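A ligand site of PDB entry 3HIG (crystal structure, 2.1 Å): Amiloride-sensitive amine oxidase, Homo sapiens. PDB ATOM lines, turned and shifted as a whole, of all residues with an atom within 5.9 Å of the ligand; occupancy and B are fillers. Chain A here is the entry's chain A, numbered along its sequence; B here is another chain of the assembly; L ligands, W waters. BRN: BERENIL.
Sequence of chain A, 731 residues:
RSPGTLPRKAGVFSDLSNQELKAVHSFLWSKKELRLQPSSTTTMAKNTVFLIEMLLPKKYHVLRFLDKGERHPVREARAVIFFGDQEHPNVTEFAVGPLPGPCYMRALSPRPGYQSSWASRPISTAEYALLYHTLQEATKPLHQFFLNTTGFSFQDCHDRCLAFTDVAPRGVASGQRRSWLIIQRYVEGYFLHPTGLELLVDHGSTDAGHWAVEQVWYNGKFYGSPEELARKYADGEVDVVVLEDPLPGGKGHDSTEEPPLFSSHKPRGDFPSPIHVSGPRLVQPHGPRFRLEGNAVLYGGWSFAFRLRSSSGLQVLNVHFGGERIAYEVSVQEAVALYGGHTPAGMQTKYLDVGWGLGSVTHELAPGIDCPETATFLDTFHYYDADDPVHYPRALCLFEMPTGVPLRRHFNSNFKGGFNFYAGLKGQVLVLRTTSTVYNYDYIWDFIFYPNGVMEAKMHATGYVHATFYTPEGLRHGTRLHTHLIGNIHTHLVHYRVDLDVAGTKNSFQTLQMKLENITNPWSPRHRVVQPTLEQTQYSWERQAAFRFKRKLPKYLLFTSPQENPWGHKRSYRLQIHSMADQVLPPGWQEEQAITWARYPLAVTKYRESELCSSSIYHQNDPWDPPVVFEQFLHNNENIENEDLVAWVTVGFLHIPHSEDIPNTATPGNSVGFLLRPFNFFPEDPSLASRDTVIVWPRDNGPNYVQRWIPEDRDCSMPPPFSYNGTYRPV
The side-chain carboxylate (OD1) of Asp 353 lies within salt-bridge range of a nitrogen (NA') of the ligand (2.8 Å).
OD1 of Asp 166 lies within hydrogen-bond range of N1 of the ligand.
OH of Tyr 351 is in hydrogen-bond range of O of Asp 166 (2.7 Å).
The side-chain carboxylate of Asp 166 is in hydrogen-bond range of the side-chain hydroxyl of Tyr 128 (2.8 Å).
The indole nitrogen of Trp 356 is in hydrogen-bond range of the side-chain amide oxygen of Gln 620, at 3.0 Å.
OG1 of Thr 165 sits at hydrogen-bond distance from OH of Tyr 439 (2.5 Å).
The backbone NH (N) of Phe 164 sits at hydrogen-bond distance from the side-chain hydroxyl (OH) of Tyr 132, 3.3 Å away.
ND2 of Asn 440 lies within hydrogen-bond range of O2 of TPQ 441.
The side-chain amide nitrogen of Asn 440 sits close to the backbone NH of His 466 (3.4 Å).
NE1 of Trp 356 lies close to NA' of the ligand (3.1 Å).
Tyr 128 touches the ligand.
Tyr 132 touches the ligand (CE2 to NB, 3.9 Å).
Phe 164 touches the ligand (O to C6, 3.3 Å).
Thr 165 touches the ligand (CG2 to N1', 3.7 Å).
Tyr 351 touches the ligand (OH to C6', 3.2 Å).
CG1 of Val 438 touches C3' of the ligand, at 3.6 Å.
CD2 of Tyr 439 touches C6' of the ligand, 3.3 Å away.
Asn 440 touches the ligand (OD1 to C5', 3.8 Å).
CB of Phe 415 of chain B touches NA of the ligand, 3.6 Å away.
Hydrophobic or aromatic side chains that line the ligand: Tyr 128, Tyr 132, Tyr 351, Trp 356, Val 438, Tyr 439 and Phe 415 of chain B.
12 residues have an atom within 4 Å of the ligand: Tyr 128, Tyr 132, Phe 164, Thr 165, Asp 166, Tyr 351, Asp 353, Trp 356, Val 438, Tyr 439, Asn 440 and Phe 415 of chain B.
The nearest printed residue that does not touch the ligand is TPQ 441 (4.6 Å).
Water W2 lies within hydrogen-bond range of OD2 of Asp 353 (2.5 Å) and NB' of the ligand (3.0 Å).
Water W1 lies within hydrogen-bond range of the side-chain hydroxyl (OH) of Tyr 132 (2.8 Å) and a nitrogen (NB) of the ligand (3.1 Å).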
ATOM      1  N   THR A 125     -17.183  21.657  30.583  1.00  0.00           N
ATOM      2  CA  THR A 125     -17.106  22.798  31.498  1.00  0.00           C
ATOM      3  C   THR A 125     -16.469  22.434  32.857  1.00  0.00           C
ATOM      4  O   THR A 125     -15.632  23.176  33.349  1.00  0.00           O
ATOM      5  CB  THR A 125     -18.497  23.415  31.699  1.00  0.00           C
ATOM      6  OG1 THR A 125     -18.888  24.009  30.456  1.00  0.00           O
ATOM      7  CG2 THR A 125     -18.467  24.475  32.749  1.00  0.00           C
ATOM      8  N   TYR A 128     -12.714  22.162  32.368  1.00  0.00           N
ATOM      9  CA  TYR A 128     -12.077  23.488  32.217  1.00  0.00           C
ATOM     10  C   TYR A 128     -11.858  24.161  33.586  1.00  0.00           C
ATOM     11  O   TYR A 128     -10.777  24.751  33.847  1.00  0.00           O
ATOM     12  CB  TYR A 128     -12.902  24.418  31.298  1.00  0.00           C
ATOM     13  CG  TYR A 128     -12.682  24.231  29.787  1.00  0.00           C
ATOM     14  CD1 TYR A 128     -11.419  24.411  29.219  1.00  0.00           C
ATOM     15  CD2 TYR A 128     -13.737  23.924  28.923  1.00  0.00           C
ATOM     16  CE1 TYR A 128     -11.209  24.263  27.850  1.00  0.00           C
ATOM     17  CE2 TYR A 128     -13.547  23.782  27.562  1.00  0.00           C
ATOM     18  CZ  TYR A 128     -12.273  23.962  27.022  1.00  0.00           C
ATOM     19  OH  TYR A 128     -12.062  23.792  25.674  1.00  0.00           O
ATOM     20  N   TYR A 132      -8.381  25.258  35.222  1.00  0.00           N
ATOM     21  CA  TYR A 132      -8.088  26.559  35.816  1.00  0.00           C
ATOM     22  C   TYR A 132      -7.451  26.427  37.210  1.00  0.00           C
ATOM     23  O   TYR A 132      -6.529  27.168  37.543  1.00  0.00           O
ATOM     24  CB  TYR A 132      -9.326  27.452  35.837  1.00  0.00           C
ATOM     25  CG  TYR A 132      -9.393  28.328  34.617  1.00  0.00           C
ATOM     26  CD1 TYR A 132      -8.520  29.410  34.494  1.00  0.00           C
ATOM     27  CD2 TYR A 132     -10.290  28.071  33.569  1.00  0.00           C
ATOM     28  CE1 TYR A 132      -8.548  30.228  33.334  1.00  0.00           C
ATOM     29  CE2 TYR A 132     -10.335  28.875  32.404  1.00  0.00           C
ATOM     30  CZ  TYR A 132      -9.459  29.957  32.290  1.00  0.00           C
ATOM     31  OH  TYR A 132      -9.479  30.767  31.170  1.00  0.00           O
ATOM     32  N   PHE A 164      -6.793  31.036  29.270  1.00  0.00           N
ATOM     33  CA  PHE A 164      -6.157  30.181  28.267  1.00  0.00           C
ATOM     34  C   PHE A 164      -7.131  29.704  27.179  1.00  0.00           C
ATOM     35  O   PHE A 164      -8.329  29.589  27.394  1.00  0.00           O
ATOM     36  CB  PHE A 164      -5.480  28.963  28.905  1.00  0.00           C
ATOM     37  CG  PHE A 164      -6.433  28.023  29.561  1.00  0.00           C
ATOM     38  CD1 PHE A 164      -6.774  28.177  30.882  1.00  0.00           C
ATOM     39  CD2 PHE A 164      -7.003  26.981  28.828  1.00  0.00           C
ATOM     40  CE1 PHE A 164      -7.662  27.310  31.472  1.00  0.00           C
ATOM     41  CE2 PHE A 164      -7.878  26.115  29.413  1.00  0.00           C
ATOM     42  CZ  PHE A 164      -8.219  26.269  30.734  1.00  0.00           C
ATOM     43  N   THR A 165      -6.569  29.452  25.999  1.00  0.00           N
ATOM     44  CA  THR A 165      -7.279  28.791  24.897  1.00  0.00           C
ATOM     45  C   THR A 165      -6.651  27.412  24.794  1.00  0.00           C
ATOM     46  O   THR A 165      -5.440  27.313  24.678  1.00  0.00           O
ATOM     47  CB  THR A 165      -7.048  29.610  23.599  1.00  0.00           C
ATOM     48  OG1 THR A 165      -7.784  30.845  23.685  1.00  0.00           O
ATOM     49  CG2 THR A 165      -7.484  28.851  22.352  1.00  0.00           C
ATOM     50  N   ASP A 166      -7.431  26.333  24.883  1.00  0.00           N
ATOM     51  CA  ASP A 166      -6.802  25.006  24.685  1.00  0.00           C
ATOM     52  C   ASP A 166      -6.778  24.609  23.221  1.00  0.00           C
ATOM     53  O   ASP A 166      -7.558  25.071  22.386  1.00  0.00           O
ATOM     54  CB  ASP A 166      -7.435  23.878  25.519  1.00  0.00           C
ATOM     55  CG  ASP A 166      -8.871  23.671  25.202  1.00  0.00           C
ATOM     56  OD1 ASP A 166      -9.543  24.689  24.953  1.00  0.00           O
ATOM     57  OD2 ASP A 166      -9.327  22.509  25.203  1.00  0.00           O
ATOM     58  N   VAL A 167      -5.823  23.758  22.922  1.00  0.00           N
ATOM     59  CA  VAL A 167      -5.573  23.334  21.577  1.00  0.00           C
ATOM     60  C   VAL A 167      -5.798  21.829  21.584  1.00  0.00           C
ATOM     61  O   VAL A 167      -5.519  21.162  22.579  1.00  0.00           O
ATOM     62  CB  VAL A 167      -4.136  23.727  21.172  1.00  0.00           C
ATOM     63  CG1 VAL A 167      -3.606  22.821  20.100  1.00  0.00           C
ATOM     64  CG2 VAL A 167      -4.096  25.209  20.742  1.00  0.00           C
ATOM     65  N   TYR A 351      -8.184  21.489  14.752  1.00  0.00           N
ATOM     66  CA  TYR A 351      -9.520  21.477  15.339  1.00  0.00           C
ATOM     67  C   TYR A 351     -10.522  20.733  14.460  1.00  0.00           C
ATOM     68  O   TYR A 351     -10.619  21.013  13.274  1.00  0.00           O
ATOM     69  CB  TYR A 351     -10.018  22.897  15.554  1.00  0.00           C
ATOM     70  CG  TYR A 351      -9.330  23.651  16.665  1.00  0.00           C
ATOM     71  CD1 TYR A 351      -9.307  23.141  17.960  1.00  0.00           C
ATOM     72  CD2 TYR A 351      -8.779  24.905  16.439  1.00  0.00           C
ATOM     73  CE1 TYR A 351      -8.690  23.851  19.001  1.00  0.00           C
ATOM     74  CE2 TYR A 351      -8.165  25.630  17.471  1.00  0.00           C
ATOM     75  CZ  TYR A 351      -8.119  25.093  18.746  1.00  0.00           C
ATOM     76  OH  TYR A 351      -7.537  25.775  19.768  1.00  0.00           O
ATOM     77  N   LEU A 352     -11.259  19.805  15.068  1.00  0.00           N
ATOM     78  CA  LEU A 352     -12.382  19.103  14.458  1.00  0.00           C
ATOM     79  C   LEU A 352     -13.653  19.447  15.272  1.00  0.00           C
ATOM     80  O   LEU A 352     -13.820  18.986  16.402  1.00  0.00           O
ATOM     81  CB  LEU A 352     -12.143  17.593  14.497  1.00  0.00           C
ATOM     82  CG  LEU A 352     -11.255  16.949  13.436  1.00  0.00           C
ATOM     83  CD1 LEU A 352      -9.849  17.501  13.492  1.00  0.00           C
ATOM     84  CD2 LEU A 352     -11.271  15.403  13.599  1.00  0.00           C
ATOM     85  N   ASP A 353     -14.541  20.248  14.683  1.00  0.00           N
ATOM     86  CA  ASP A 353     -15.576  20.917  15.446  1.00  0.00           C
ATOM     87  C   ASP A 353     -16.708  20.025  15.966  1.00  0.00           C
ATOM     88  O   ASP A 353     -17.364  20.393  16.938  1.00  0.00           O
ATOM     89  CB  ASP A 353     -16.170  22.082  14.660  1.00  0.00           C
ATOM     90  CG  ASP A 353     -15.293  23.352  14.708  1.00  0.00           C
ATOM     91  OD1 ASP A 353     -14.171  23.326  15.318  1.00  0.00           O
ATOM     92  OD2 ASP A 353     -15.744  24.360  14.132  1.00  0.00           O
ATOM     93  N   TRP A 356     -16.749  19.223  19.486  1.00  0.00           N
ATOM     94  CA  TRP A 356     -17.137  20.290  20.422  1.00  0.00           C
ATOM     95  C   TRP A 356     -18.611  20.613  20.415  1.00  0.00           C
ATOM     96  O   TRP A 356     -19.034  21.609  21.023  1.00  0.00           O
ATOM     97  CB  TRP A 356     -16.391  21.552  20.071  1.00  0.00           C
ATOM     98  CG  TRP A 356     -14.940  21.377  20.047  1.00  0.00           C
ATOM     99  CD1 TRP A 356     -14.191  20.843  19.028  1.00  0.00           C
ATOM    100  CD2 TRP A 356     -14.031  21.727  21.071  1.00  0.00           C
ATOM    101  NE1 TRP A 356     -12.864  20.863  19.361  1.00  0.00           N
ATOM    102  CE2 TRP A 356     -12.736  21.403  20.611  1.00  0.00           C
ATOM    103  CE3 TRP A 356     -14.182  22.324  22.329  1.00  0.00           C
ATOM    104  CZ2 TRP A 356     -11.601  21.621  21.380  1.00  0.00           C
ATOM    105  CZ3 TRP A 356     -13.050  22.529  23.088  1.00  0.00           C
ATOM    106  CH2 TRP A 356     -11.775  22.191  22.614  1.00  0.00           C
ATOM    107  N   VAL A 438     -18.154  27.890  18.172  1.00  0.00           N
ATOM    108  CA  VAL A 438     -17.599  26.993  19.223  1.00  0.00           C
ATOM    109  C   VAL A 438     -16.721  27.803  20.180  1.00  0.00           C
ATOM    110  O   VAL A 438     -16.769  27.612  21.410  1.00  0.00           O
ATOM    111  CB  VAL A 438     -16.765  25.857  18.633  1.00  0.00           C
ATOM    112  CG1 VAL A 438     -16.038  25.082  19.771  1.00  0.00           C
ATOM    113  CG2 VAL A 438     -17.656  24.924  17.774  1.00  0.00           C
ATOM    114  N   TYR A 439     -15.926  28.710  19.625  1.00  0.00           N
ATOM    115  CA  TYR A 439     -15.034  29.524  20.417  1.00  0.00           C
ATOM    116  C   TYR A 439     -14.760  30.860  19.750  1.00  0.00           C
ATOM    117  O   TYR A 439     -15.467  31.844  20.036  1.00  0.00           O
ATOM    118  CB  TYR A 439     -13.760  28.737  20.704  1.00  0.00           C
ATOM    119  CG  TYR A 439     -12.804  29.350  21.694  1.00  0.00           C
ATOM    120  CD1 TYR A 439     -13.167  29.475  23.033  1.00  0.00           C
ATOM    121  CD2 TYR A 439     -11.523  29.753  21.314  1.00  0.00           C
ATOM    122  CE1 TYR A 439     -12.274  30.017  23.970  1.00  0.00           C
ATOM    123  CE2 TYR A 439     -10.634  30.289  22.221  1.00  0.00           C
ATOM    124  CZ  TYR A 439     -11.017  30.413  23.546  1.00  0.00           C
ATOM    125  OH  TYR A 439     -10.153  30.934  24.462  1.00  0.00           O
ATOM    126  N   ASN A 440     -13.792  30.908  18.841  1.00  0.00           N
ATOM    127  CA  ASN A 440     -13.352  32.169  18.230  1.00  0.00           C
ATOM    128  C   ASN A 440     -14.061  32.460  16.918  1.00  0.00           C
ATOM    129  O   ASN A 440     -14.388  33.620  16.651  1.00  0.00           O
ATOM    130  CB  ASN A 440     -11.815  32.199  18.006  1.00  0.00           C
ATOM    131  CG  ASN A 440     -11.292  30.997  17.242  1.00  0.00           C
ATOM    132  OD1 ASN A 440     -11.436  29.859  17.682  1.00  0.00           O
ATOM    133  ND2 ASN A 440     -10.684  31.248  16.084  1.00  0.00           N
ATOM    134  N   TPQ A 441     -14.242  31.428  16.095  1.00  0.00           N
ATOM    135  CA  TPQ A 441     -14.874  31.537  14.773  1.00  0.00           C
ATOM    136  CB  TPQ A 441     -14.392  30.408  13.822  1.00  0.00           C
ATOM    137  C   TPQ A 441     -16.394  31.419  14.851  1.00  0.00           C
ATOM    138  O   TPQ A 441     -16.919  30.654  15.661  1.00  0.00           O
ATOM    139  C1  TPQ A 441     -13.163  30.827  13.036  1.00  0.00           C
ATOM    140  C2  TPQ A 441     -11.951  29.981  13.089  1.00  0.00           C
ATOM    141  O2  TPQ A 441     -11.920  28.933  13.787  1.00  0.00           O
ATOM    142  C3  TPQ A 441     -10.755  30.391  12.315  1.00  0.00           C
ATOM    143  C4  TPQ A 441     -10.762  31.555  11.525  1.00  0.00           C
ATOM    144  O4  TPQ A 441      -9.763  31.894  10.886  1.00  0.00           O
ATOM    145  C5  TPQ A 441     -11.978  32.401  11.463  1.00  0.00           C
ATOM    146  O5  TPQ A 441     -11.978  33.436  10.764  1.00  0.00           O
ATOM    147  C6  TPQ A 441     -13.170  31.977  12.246  1.00  0.00           C
ATOM    148  N   HIS A 466      -7.559  32.192  15.046  1.00  0.00           N
ATOM    149  CA  HIS A 466      -6.689  31.489  15.983  1.00  0.00           C
ATOM    150  C   HIS A 466      -5.280  32.088  15.805  1.00  0.00           C
ATOM    151  O   HIS A 466      -4.692  32.005  14.713  1.00  0.00           O
ATOM    152  CB  HIS A 466      -6.752  29.995  15.653  1.00  0.00           C
ATOM    153  CG  HIS A 466      -5.998  29.105  16.588  1.00  0.00           C
ATOM    154  ND1 HIS A 466      -6.310  28.990  17.926  1.00  0.00           N
ATOM    155  CD2 HIS A 466      -4.992  28.233  16.365  1.00  0.00           C
ATOM    156  CE1 HIS A 466      -5.511  28.110  18.493  1.00  0.00           C
ATOM    157  NE2 HIS A 466      -4.702  27.632  17.560  1.00  0.00           N
ATOM    158  N   GLN A 620     -11.868  14.292  17.404  1.00  0.00           N
ATOM    159  CA  GLN A 620     -10.977  15.398  17.807  1.00  0.00           C
ATOM    160  C   GLN A 620      -9.876  14.961  18.759  1.00  0.00           C
ATOM    161  O   GLN A 620      -8.729  15.363  18.610  1.00  0.00           O
ATOM    162  CB  GLN A 620     -11.766  16.520  18.476  1.00  0.00           C
ATOM    163  CG  GLN A 620     -10.905  17.641  19.103  1.00  0.00           C
ATOM    164  CD  GLN A 620     -10.192  18.514  18.077  1.00  0.00           C
ATOM    165  OE1 GLN A 620     -10.646  19.636  17.770  1.00  0.00           O
ATOM    166  NE2 GLN A 620      -9.065  18.047  17.559  1.00  0.00           N
ATOM    167  N   ASN B 414     -19.848  33.644  27.396  1.00  0.00           N
ATOM    168  CA  ASN B 414     -19.125  33.467  28.672  1.00  0.00           C
ATOM    169  C   ASN B 414     -19.033  31.988  29.095  1.00  0.00           C
ATOM    170  O   ASN B 414     -18.523  31.691  30.172  1.00  0.00           O
ATOM    171  CB  ASN B 414     -19.688  34.371  29.777  1.00  0.00           C
ATOM    172  CG  ASN B 414     -21.089  34.000  30.223  1.00  0.00           C
ATOM    173  OD1 ASN B 414     -21.644  32.949  29.857  1.00  0.00           O
ATOM    174  ND2 ASN B 414     -21.664  34.853  31.043  1.00  0.00           N
ATOM    175  N   PHE B 415     -19.530  31.084  28.263  1.00  0.00           N
ATOM    176  CA  PHE B 415     -19.543  29.641  28.544  1.00  0.00           C
ATOM    177  C   PHE B 415     -20.203  29.286  29.879  1.00  0.00           C
ATOM    178  O   PHE B 415     -19.914  28.232  30.460  1.00  0.00           O
ATOM    179  CB  PHE B 415     -18.102  29.100  28.465  1.00  0.00           C
ATOM    180  CG  PHE B 415     -17.406  29.497  27.192  1.00  0.00           C
ATOM    181  CD1 PHE B 415     -16.484  30.528  27.177  1.00  0.00           C
ATOM    182  CD2 PHE B 415     -17.744  28.888  25.996  1.00  0.00           C
ATOM    183  CE1 PHE B 415     -15.860  30.922  25.995  1.00  0.00           C
ATOM    184  CE2 PHE B 415     -17.116  29.260  24.801  1.00  0.00           C
ATOM    185  CZ  PHE B 415     -16.208  30.291  24.792  1.00  0.00           C
HETATM  186  C1  BRN L   1     -11.634  27.388  25.976  1.00  0.00           C
HETATM  187  C2  BRN L   1     -13.026  27.262  25.910  1.00  0.00           C
HETATM  188  C3  BRN L   1     -13.811  27.489  27.033  1.00  0.00           C
HETATM  189  C4  BRN L   1     -13.214  27.728  28.267  1.00  0.00           C
HETATM  190  C5  BRN L   1     -11.829  27.853  28.356  1.00  0.00           C
HETATM  191  C6  BRN L   1     -11.045  27.676  27.213  1.00  0.00           C
HETATM  192  C7  BRN L   1     -14.077  27.901  29.482  1.00  0.00           C
HETATM  193  NA  BRN L   1     -15.188  27.318  29.551  1.00  0.00           N
HETATM  194  NB  BRN L   1     -13.753  28.742  30.451  1.00  0.00           N
HETATM  195  N1  BRN L   1     -10.844  27.224  24.894  1.00  0.00           N
HETATM  196  N   BRN L   1     -11.307  26.838  23.705  1.00  0.00           N
HETATM  197  N1' BRN L   1     -10.516  26.721  22.731  1.00  0.00           N
HETATM  198  C1' BRN L   1     -10.996  26.329  21.474  1.00  0.00           C
HETATM  199  C2' BRN L   1     -11.969  25.333  21.454  1.00  0.00           C
HETATM  200  C3' BRN L   1     -12.464  24.876  20.255  1.00  0.00           C
HETATM  201  C4' BRN L   1     -12.036  25.394  19.040  1.00  0.00           C
HETATM  202  C5' BRN L   1     -11.060  26.383  19.047  1.00  0.00           C
HETATM  203  C6' BRN L   1     -10.531  26.841  20.256  1.00  0.00           C
HETATM  204  C7' BRN L   1     -12.642  24.815  17.794  1.00  0.00           C
HETATM  205  NA' BRN L   1     -12.943  23.577  17.822  1.00  0.00           N
HETATM  206  NB' BRN L   1     -12.777  25.524  16.682  1.00  0.00           N
HETATM  207  O   HOH W   1     -11.869  31.126  29.677  1.00  0.00           O
HETATM  208  O   HOH W   2     -14.814  26.601  14.751  1.00  0.00           O
HETATM  209  O   HOH W   3     -15.432  29.659  32.766  1.00  0.00           O
HETATM  210  O   HOH W   4     -16.456  25.516  27.965  1.00  0.00           O
